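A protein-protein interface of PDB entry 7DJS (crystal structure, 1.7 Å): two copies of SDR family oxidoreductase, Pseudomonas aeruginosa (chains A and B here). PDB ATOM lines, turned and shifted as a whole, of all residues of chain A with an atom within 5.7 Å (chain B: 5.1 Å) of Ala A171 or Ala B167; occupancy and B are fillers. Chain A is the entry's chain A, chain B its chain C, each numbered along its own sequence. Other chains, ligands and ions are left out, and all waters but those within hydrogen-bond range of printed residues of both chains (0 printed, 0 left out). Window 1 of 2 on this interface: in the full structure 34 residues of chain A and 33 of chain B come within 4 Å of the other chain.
The backbone carbonyl oxygen (O) of Ala A166 lies within hydrogen-bond range of a ring nitrogen (ND1) of His A170, at 2.9 Å.
O of Ala B166 lies within hydrogen-bond range of ND1 of His B170 (2.9 Å).
The backbone carbonyl oxygen (O) of Ala B154 is in hydrogen-bond range of a ring nitrogen (ND1) of His B170.
The side-chain hydroxyl of Ser A178 lies within hydrogen-bond range of the backbone carbonyl oxygen of Gly A174 (2.9 Å).
Among the printed residues, pairs that only touch across the chains: His A170 with His B170, Ser A178 with Ala B166, Ala A167 with Ala B171, Ala A171 with Ala B167, Gly A174 with His B170, Ser A178 with Ser B163, Leu A175 with Ala B167, Leu A175 with Ser B163, Val A125 with Met B121 and His A170 with Ala B171.
Of chain B, only Ala B167 comes within 4 Å of Ala A171.
Of chain A, only Ala A171 (3.4 Å) and Leu A175 (3.6 Å) come within 4 Å of Ala B167.
Printed residues of chain B within 4 Å of Ser A178: Ser B163 and Ala B166.
Of the printed residues of chain B, Gly A174 touches His B170 (3.4 Å).
Of the printed residues of chain B, His A170 touches His B170 (3.2 Å) and Ala B171 (3.98 Å).
Of the printed residues of chain A, Ala B166 touches Ser A178 (3.3 Å).
Of the printed residues of chain A, Ser B163 touches Leu A175 (3.7 Å) and Ser A178 (3.6 Å).
The nearest residue of chain B that does not touch Ala A171 is His B170 (4.02 Å).
The nearest printed residue of chain A that does not touch Met B121 is Ala A171 (4.7 Å).
Of the 13 printed residues of chain A, 7 touch a printed residue of chain B.
Hydrophobic or aromatic side chains of chain A that line the printed part of chain B: Val A125, Ala A167, His A170, Ala A171 and Leu A175.
Of the 12 printed residues of chain B, 6 touch a printed residue of chain A.
Printed residues of chain B that touch a printed residue of chain A: Met B121, Ser B163, Ala B166, Ala B167, His B170 and Ala B171.
Hydrophobic or aromatic side chains of chain B that line the printed part of chain A: Met B121, Ala B166, Ala B167, His B170 and Ala B171.
Among the printed residues, 10 pairs touch across the chains.
Among the printed residues, no Asp or Glu carboxylate lies within 4 Å of a Lys or Arg side-chain nitrogen of the other chain.
Ala A167 touches Ala B171, and with the chains exchanged Ala A171 touches Ala B167.
His A170 touches its own counterpart, His B170.
His A170 touches Ala B171, but with the chains exchanged Ala A171 does not touch His B170 (4.02 Å).
Positions printed for both chains: 166, 167, 168, 169, 170 and 171.
Of the 10 pairs that touch across the chains among the printed residues, 3 have their exchanged pair printed and touching as well.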
ATOM      1  N   VAL A 125       7.850   5.745  -4.517  1.00  0.00           N
ATOM      2  CA  VAL A 125       7.049   4.736  -5.203  1.00  0.00           C
ATOM      3  C   VAL A 125       7.623   3.344  -4.991  1.00  0.00           C
ATOM      4  O   VAL A 125       6.950   2.468  -4.456  1.00  0.00           O
ATOM      5  CB  VAL A 125       6.887   5.051  -6.706  1.00  0.00           C
ATOM      6  CG1 VAL A 125       5.844   4.111  -7.320  1.00  0.00           C
ATOM      7  CG2 VAL A 125       6.483   6.502  -6.908  1.00  0.00           C
ATOM      8  N   ALA A 166       4.701  15.080  -7.124  1.00  0.00           N
ATOM      9  CA  ALA A 166       3.281  14.835  -7.353  1.00  0.00           C
ATOM     10  C   ALA A 166       3.067  13.529  -8.105  1.00  0.00           C
ATOM     11  O   ALA A 166       2.167  12.751  -7.760  1.00  0.00           O
ATOM     12  CB  ALA A 166       2.659  16.012  -8.108  1.00  0.00           C
ATOM     13  N   ALA A 167       3.875  13.275  -9.142  1.00  0.00           N
ATOM     14  CA  ALA A 167       3.770  12.002  -9.845  1.00  0.00           C
ATOM     15  C   ALA A 167       3.948  10.842  -8.870  1.00  0.00           C
ATOM     16  O   ALA A 167       3.190   9.863  -8.909  1.00  0.00           O
ATOM     17  CB  ALA A 167       4.812  11.926 -10.963  1.00  0.00           C
ATOM     18  N   SER A 168       4.917  10.962  -7.956  1.00  0.00           N
ATOM     19  CA  SER A 168       5.195   9.859  -7.043  1.00  0.00           C
ATOM     20  C   SER A 168       4.042   9.641  -6.069  1.00  0.00           C
ATOM     21  O   SER A 168       3.705   8.495  -5.743  1.00  0.00           O
ATOM     22  CB  SER A 168       6.510  10.101  -6.296  1.00  0.00           C
ATOM     23  OG  SER A 168       6.376  11.023  -5.221  1.00  0.00           O
ATOM     24  N   LYS A 169       3.414  10.716  -5.607  1.00  0.00           N
ATOM     25  CA  LYS A 169       2.349  10.542  -4.622  1.00  0.00           C
ATOM     26  C   LYS A 169       1.035  10.126  -5.281  1.00  0.00           C
ATOM     27  O   LYS A 169       0.225   9.415  -4.659  1.00  0.00           O
ATOM     28  CB  LYS A 169       2.187  11.818  -3.804  1.00  0.00           C
ATOM     29  CG  LYS A 169       3.412  12.158  -2.957  1.00  0.00           C
ATOM     30  CD  LYS A 169       3.797  10.998  -2.025  1.00  0.00           C
ATOM     31  CE  LYS A 169       4.758  11.465  -0.906  1.00  0.00           C
ATOM     32  NZ  LYS A 169       4.903  10.399   0.147  1.00  0.00           N
ATOM     33  N   HIS A 170       0.811  10.546  -6.529  1.00  0.00           N
ATOM     34  CA  HIS A 170      -0.250   9.941  -7.331  1.00  0.00           C
ATOM     35  C   HIS A 170      -0.035   8.435  -7.443  1.00  0.00           C
ATOM     36  O   HIS A 170      -0.967   7.645  -7.260  1.00  0.00           O
ATOM     37  CB  HIS A 170      -0.283  10.569  -8.735  1.00  0.00           C
ATOM     38  CG  HIS A 170      -1.073  11.840  -8.831  1.00  0.00           C
ATOM     39  ND1 HIS A 170      -0.648  13.036  -8.290  1.00  0.00           N
ATOM     40  CD2 HIS A 170      -2.250  12.106  -9.448  1.00  0.00           C
ATOM     41  CE1 HIS A 170      -1.537  13.980  -8.556  1.00  0.00           C
ATOM     42  NE2 HIS A 170      -2.514  13.445  -9.264  1.00  0.00           N
ATOM     43  N   ALA A 171       1.205   8.025  -7.732  1.00  0.00           N
ATOM     44  CA  ALA A 171       1.511   6.604  -7.880  1.00  0.00           C
ATOM     45  C   ALA A 171       1.214   5.833  -6.599  1.00  0.00           C
ATOM     46  O   ALA A 171       0.721   4.698  -6.649  1.00  0.00           O
ATOM     47  CB  ALA A 171       2.978   6.433  -8.278  1.00  0.00           C
ATOM     48  N   VAL A 172       1.505   6.431  -5.441  1.00  0.00           N
ATOM     49  CA  VAL A 172       1.166   5.789  -4.167  1.00  0.00           C
ATOM     50  C   VAL A 172      -0.331   5.503  -4.094  1.00  0.00           C
ATOM     51  O   VAL A 172      -0.755   4.440  -3.621  1.00  0.00           O
ATOM     52  CB  VAL A 172       1.627   6.664  -2.987  1.00  0.00           C
ATOM     53  CG1 VAL A 172       1.019   6.151  -1.671  1.00  0.00           C
ATOM     54  CG2 VAL A 172       3.148   6.662  -2.893  1.00  0.00           C
ATOM     55  N   ILE A 173      -1.159   6.452  -4.546  1.00  0.00           N
ATOM     56  CA  ILE A 173      -2.603   6.225  -4.519  1.00  0.00           C
ATOM     57  C   ILE A 173      -2.997   5.085  -5.457  1.00  0.00           C
ATOM     58  O   ILE A 173      -3.869   4.269  -5.126  1.00  0.00           O
ATOM     59  CB  ILE A 173      -3.346   7.531  -4.848  1.00  0.00           C
ATOM     60  CG1 ILE A 173      -3.081   8.540  -3.722  1.00  0.00           C
ATOM     61  CG2 ILE A 173      -4.838   7.249  -5.023  1.00  0.00           C
ATOM     62  CD1 ILE A 173      -3.627   9.916  -4.000  1.00  0.00           C
ATOM     63  N   GLY A 174      -2.360   5.000  -6.633  1.00  0.00           N
ATOM     64  CA  GLY A 174      -2.631   3.887  -7.533  1.00  0.00           C
ATOM     65  C   GLY A 174      -2.255   2.542  -6.936  1.00  0.00           C
ATOM     66  O   GLY A 174      -3.008   1.566  -7.048  1.00  0.00           O
ATOM     67  N   LEU A 175      -1.094   2.469  -6.279  1.00  0.00           N
ATOM     68  CA  LEU A 175      -0.737   1.239  -5.560  1.00  0.00           C
ATOM     69  C   LEU A 175      -1.760   0.916  -4.489  1.00  0.00           C
ATOM     70  O   LEU A 175      -2.148  -0.245  -4.312  1.00  0.00           O
ATOM     71  CB  LEU A 175       0.634   1.374  -4.908  1.00  0.00           C
ATOM     72  CG  LEU A 175       1.834   1.506  -5.838  1.00  0.00           C
ATOM     73  CD1 LEU A 175       3.085   1.801  -5.001  1.00  0.00           C
ATOM     74  CD2 LEU A 175       2.009   0.252  -6.702  1.00  0.00           C
ATOM     75  N   THR A 176      -2.179   1.938  -3.746  1.00  0.00           N
ATOM     76  CA  THR A 176      -3.092   1.762  -2.623  1.00  0.00           C
ATOM     77  C   THR A 176      -4.431   1.208  -3.081  1.00  0.00           C
ATOM     78  O   THR A 176      -4.938   0.222  -2.526  1.00  0.00           O
ATOM     79  CB  THR A 176      -3.299   3.111  -1.929  1.00  0.00           C
ATOM     80  OG1 THR A 176      -2.056   3.595  -1.407  1.00  0.00           O
ATOM     81  CG2 THR A 176      -4.315   2.972  -0.787  1.00  0.00           C
ATOM     82  N   SER A 178      -5.243  -0.223  -5.922  1.00  0.00           N
ATOM     83  CA  SER A 178      -5.136  -1.511  -6.594  1.00  0.00           C
ATOM     84  C   SER A 178      -4.973  -2.640  -5.588  1.00  0.00           C
ATOM     85  O   SER A 178      -5.680  -3.652  -5.663  1.00  0.00           O
ATOM     86  CB  SER A 178      -3.978  -1.492  -7.591  1.00  0.00           C
ATOM     87  OG  SER A 178      -4.220  -0.544  -8.617  1.00  0.00           O
ATOM     88  N   MET B 121       7.661   1.425 -14.952  1.00  0.00           N
ATOM     89  CA  MET B 121       7.901   2.803 -14.541  1.00  0.00           C
ATOM     90  C   MET B 121       8.807   3.548 -15.522  1.00  0.00           C
ATOM     91  O   MET B 121       8.596   4.746 -15.761  1.00  0.00           O
ATOM     92  CB  MET B 121       8.464   2.853 -13.120  1.00  0.00           C
ATOM     93  CG  MET B 121       7.492   2.361 -12.055  1.00  0.00           C
ATOM     94  SD  MET B 121       6.041   3.432 -11.799  1.00  0.00           S
ATOM     95  CE  MET B 121       6.508   5.032 -11.084  1.00  0.00           C
ATOM     96  N   ALA B 154      -6.965   3.232 -15.281  1.00  0.00           N
ATOM     97  CA  ALA B 154      -6.117   2.789 -14.181  1.00  0.00           C
ATOM     98  C   ALA B 154      -5.342   3.929 -13.540  1.00  0.00           C
ATOM     99  O   ALA B 154      -4.680   3.704 -12.523  1.00  0.00           O
ATOM    100  CB  ALA B 154      -5.139   1.709 -14.645  1.00  0.00           C
ATOM    101  N   MET B 162      -2.823  -5.337 -11.934  1.00  0.00           N
ATOM    102  CA  MET B 162      -2.067  -4.370 -12.714  1.00  0.00           C
ATOM    103  C   MET B 162      -1.700  -3.195 -11.828  1.00  0.00           C
ATOM    104  O   MET B 162      -1.828  -2.029 -12.225  1.00  0.00           O
ATOM    105  CB  MET B 162      -2.861  -3.905 -13.937  1.00  0.00           C
ATOM    106  CG  MET B 162      -3.094  -4.988 -14.970  1.00  0.00           C
ATOM    107  SD  MET B 162      -4.144  -4.412 -16.307  1.00  0.00           S
ATOM    108  CE  MET B 162      -5.643  -4.002 -15.438  1.00  0.00           C
ATOM    109  N   SER B 163      -1.255  -3.498 -10.598  1.00  0.00           N
ATOM    110  CA  SER B 163      -1.053  -2.447  -9.605  1.00  0.00           C
ATOM    111  C   SER B 163       0.110  -1.525  -9.975  1.00  0.00           C
ATOM    112  O   SER B 163       0.043  -0.315  -9.725  1.00  0.00           O
ATOM    113  CB  SER B 163      -0.851  -3.065  -8.216  1.00  0.00           C
ATOM    114  OG  SER B 163       0.392  -3.739  -8.129  1.00  0.00           O
ATOM    115  N   ILE B 164       1.179  -2.067 -10.566  1.00  0.00           N
ATOM    116  CA  ILE B 164       2.282  -1.197 -10.994  1.00  0.00           C
ATOM    117  C   ILE B 164       1.839  -0.325 -12.160  1.00  0.00           C
ATOM    118  O   ILE B 164       2.151   0.878 -12.219  1.00  0.00           O
ATOM    119  CB  ILE B 164       3.530  -2.020 -11.375  1.00  0.00           C
ATOM    120  CG1 ILE B 164       3.976  -2.924 -10.218  1.00  0.00           C
ATOM    121  CG2 ILE B 164       4.686  -1.094 -11.785  1.00  0.00           C
ATOM    122  CD1 ILE B 164       4.975  -4.006 -10.662  1.00  0.00           C
ATOM    123  N   TYR B 165       1.120  -0.922 -13.106  1.00  0.00           N
ATOM    124  CA  TYR B 165       0.535  -0.162 -14.209  1.00  0.00           C
ATOM    125  C   TYR B 165      -0.339   0.970 -13.687  1.00  0.00           C
ATOM    126  O   TYR B 165      -0.234   2.122 -14.134  1.00  0.00           O
ATOM    127  CB  TYR B 165      -0.284  -1.098 -15.096  1.00  0.00           C
ATOM    128  CG  TYR B 165      -0.862  -0.440 -16.323  1.00  0.00           C
ATOM    129  CD1 TYR B 165      -0.067  -0.192 -17.431  1.00  0.00           C
ATOM    130  CD2 TYR B 165      -2.206  -0.072 -16.372  1.00  0.00           C
ATOM    131  CE1 TYR B 165      -0.594   0.391 -18.570  1.00  0.00           C
ATOM    132  CE2 TYR B 165      -2.741   0.515 -17.501  1.00  0.00           C
ATOM    133  CZ  TYR B 165      -1.928   0.751 -18.591  1.00  0.00           C
ATOM    134  OH  TYR B 165      -2.457   1.338 -19.715  1.00  0.00           O
ATOM    135  N   ALA B 166      -1.205   0.662 -12.718  1.00  0.00           N
ATOM    136  CA  ALA B 166      -2.048   1.707 -12.151  1.00  0.00           C
ATOM    137  C   ALA B 166      -1.204   2.782 -11.483  1.00  0.00           C
ATOM    138  O   ALA B 166      -1.458   3.980 -11.658  1.00  0.00           O
ATOM    139  CB  ALA B 166      -3.059   1.106 -11.166  1.00  0.00           C
ATOM    140  N   ALA B 167      -0.184   2.384 -10.719  1.00  0.00           N
ATOM    141  CA  ALA B 167       0.708   3.385 -10.148  1.00  0.00           C
ATOM    142  C   ALA B 167       1.302   4.266 -11.242  1.00  0.00           C
ATOM    143  O   ALA B 167       1.345   5.498 -11.105  1.00  0.00           O
ATOM    144  CB  ALA B 167       1.815   2.710  -9.334  1.00  0.00           C
ATOM    145  N   SER B 168       1.732   3.656 -12.347  1.00  0.00           N
ATOM    146  CA  SER B 168       2.380   4.431 -13.398  1.00  0.00           C
ATOM    147  C   SER B 168       1.404   5.388 -14.072  1.00  0.00           C
ATOM    148  O   SER B 168       1.775   6.514 -14.405  1.00  0.00           O
ATOM    149  CB  SER B 168       3.028   3.500 -14.424  1.00  0.00           C
ATOM    150  OG  SER B 168       2.082   2.933 -15.315  1.00  0.00           O
ATOM    151  N   LYS B 169       0.161   4.965 -14.284  1.00  0.00           N
ATOM    152  CA  LYS B 169      -0.793   5.851 -14.947  1.00  0.00           C
ATOM    153  C   LYS B 169      -1.343   6.920 -14.006  1.00  0.00           C
ATOM    154  O   LYS B 169      -1.658   8.021 -14.462  1.00  0.00           O
ATOM    155  CB  LYS B 169      -1.929   5.036 -15.568  1.00  0.00           C
ATOM    156  CG  LYS B 169      -1.435   4.161 -16.706  1.00  0.00           C
ATOM    157  CD  LYS B 169      -0.623   4.955 -17.738  1.00  0.00           C
ATOM    158  CE  LYS B 169      -0.418   4.123 -19.005  1.00  0.00           C
ATOM    159  NZ  LYS B 169      -0.047   4.975 -20.173  1.00  0.00           N
ATOM    160  N   HIS B 170      -1.470   6.620 -12.710  1.00  0.00           N
ATOM    161  CA  HIS B 170      -1.685   7.679 -11.724  1.00  0.00           C
ATOM    162  C   HIS B 170      -0.582   8.726 -11.800  1.00  0.00           C
ATOM    163  O   HIS B 170      -0.855   9.931 -11.795  1.00  0.00           O
ATOM    164  CB  HIS B 170      -1.734   7.087 -10.315  1.00  0.00           C
ATOM    165  CG  HIS B 170      -3.086   6.586  -9.906  1.00  0.00           C
ATOM    166  ND1 HIS B 170      -3.653   5.442 -10.425  1.00  0.00           N
ATOM    167  CD2 HIS B 170      -3.963   7.059  -8.986  1.00  0.00           C
ATOM    168  CE1 HIS B 170      -4.833   5.245  -9.859  1.00  0.00           C
ATOM    169  NE2 HIS B 170      -5.037   6.205  -8.973  1.00  0.00           N
ATOM    170  N   ALA B 171       0.678   8.275 -11.843  1.00  0.00           N
ATOM    171  CA  ALA B 171       1.811   9.196 -11.911  1.00  0.00           C
ATOM    172  C   ALA B 171       1.733  10.092 -13.144  1.00  0.00           C
ATOM    173  O   ALA B 171       2.078  11.283 -13.074  1.00  0.00           O
ATOM    174  CB  ALA B 171       3.123   8.398 -11.898  1.00  0.00           C
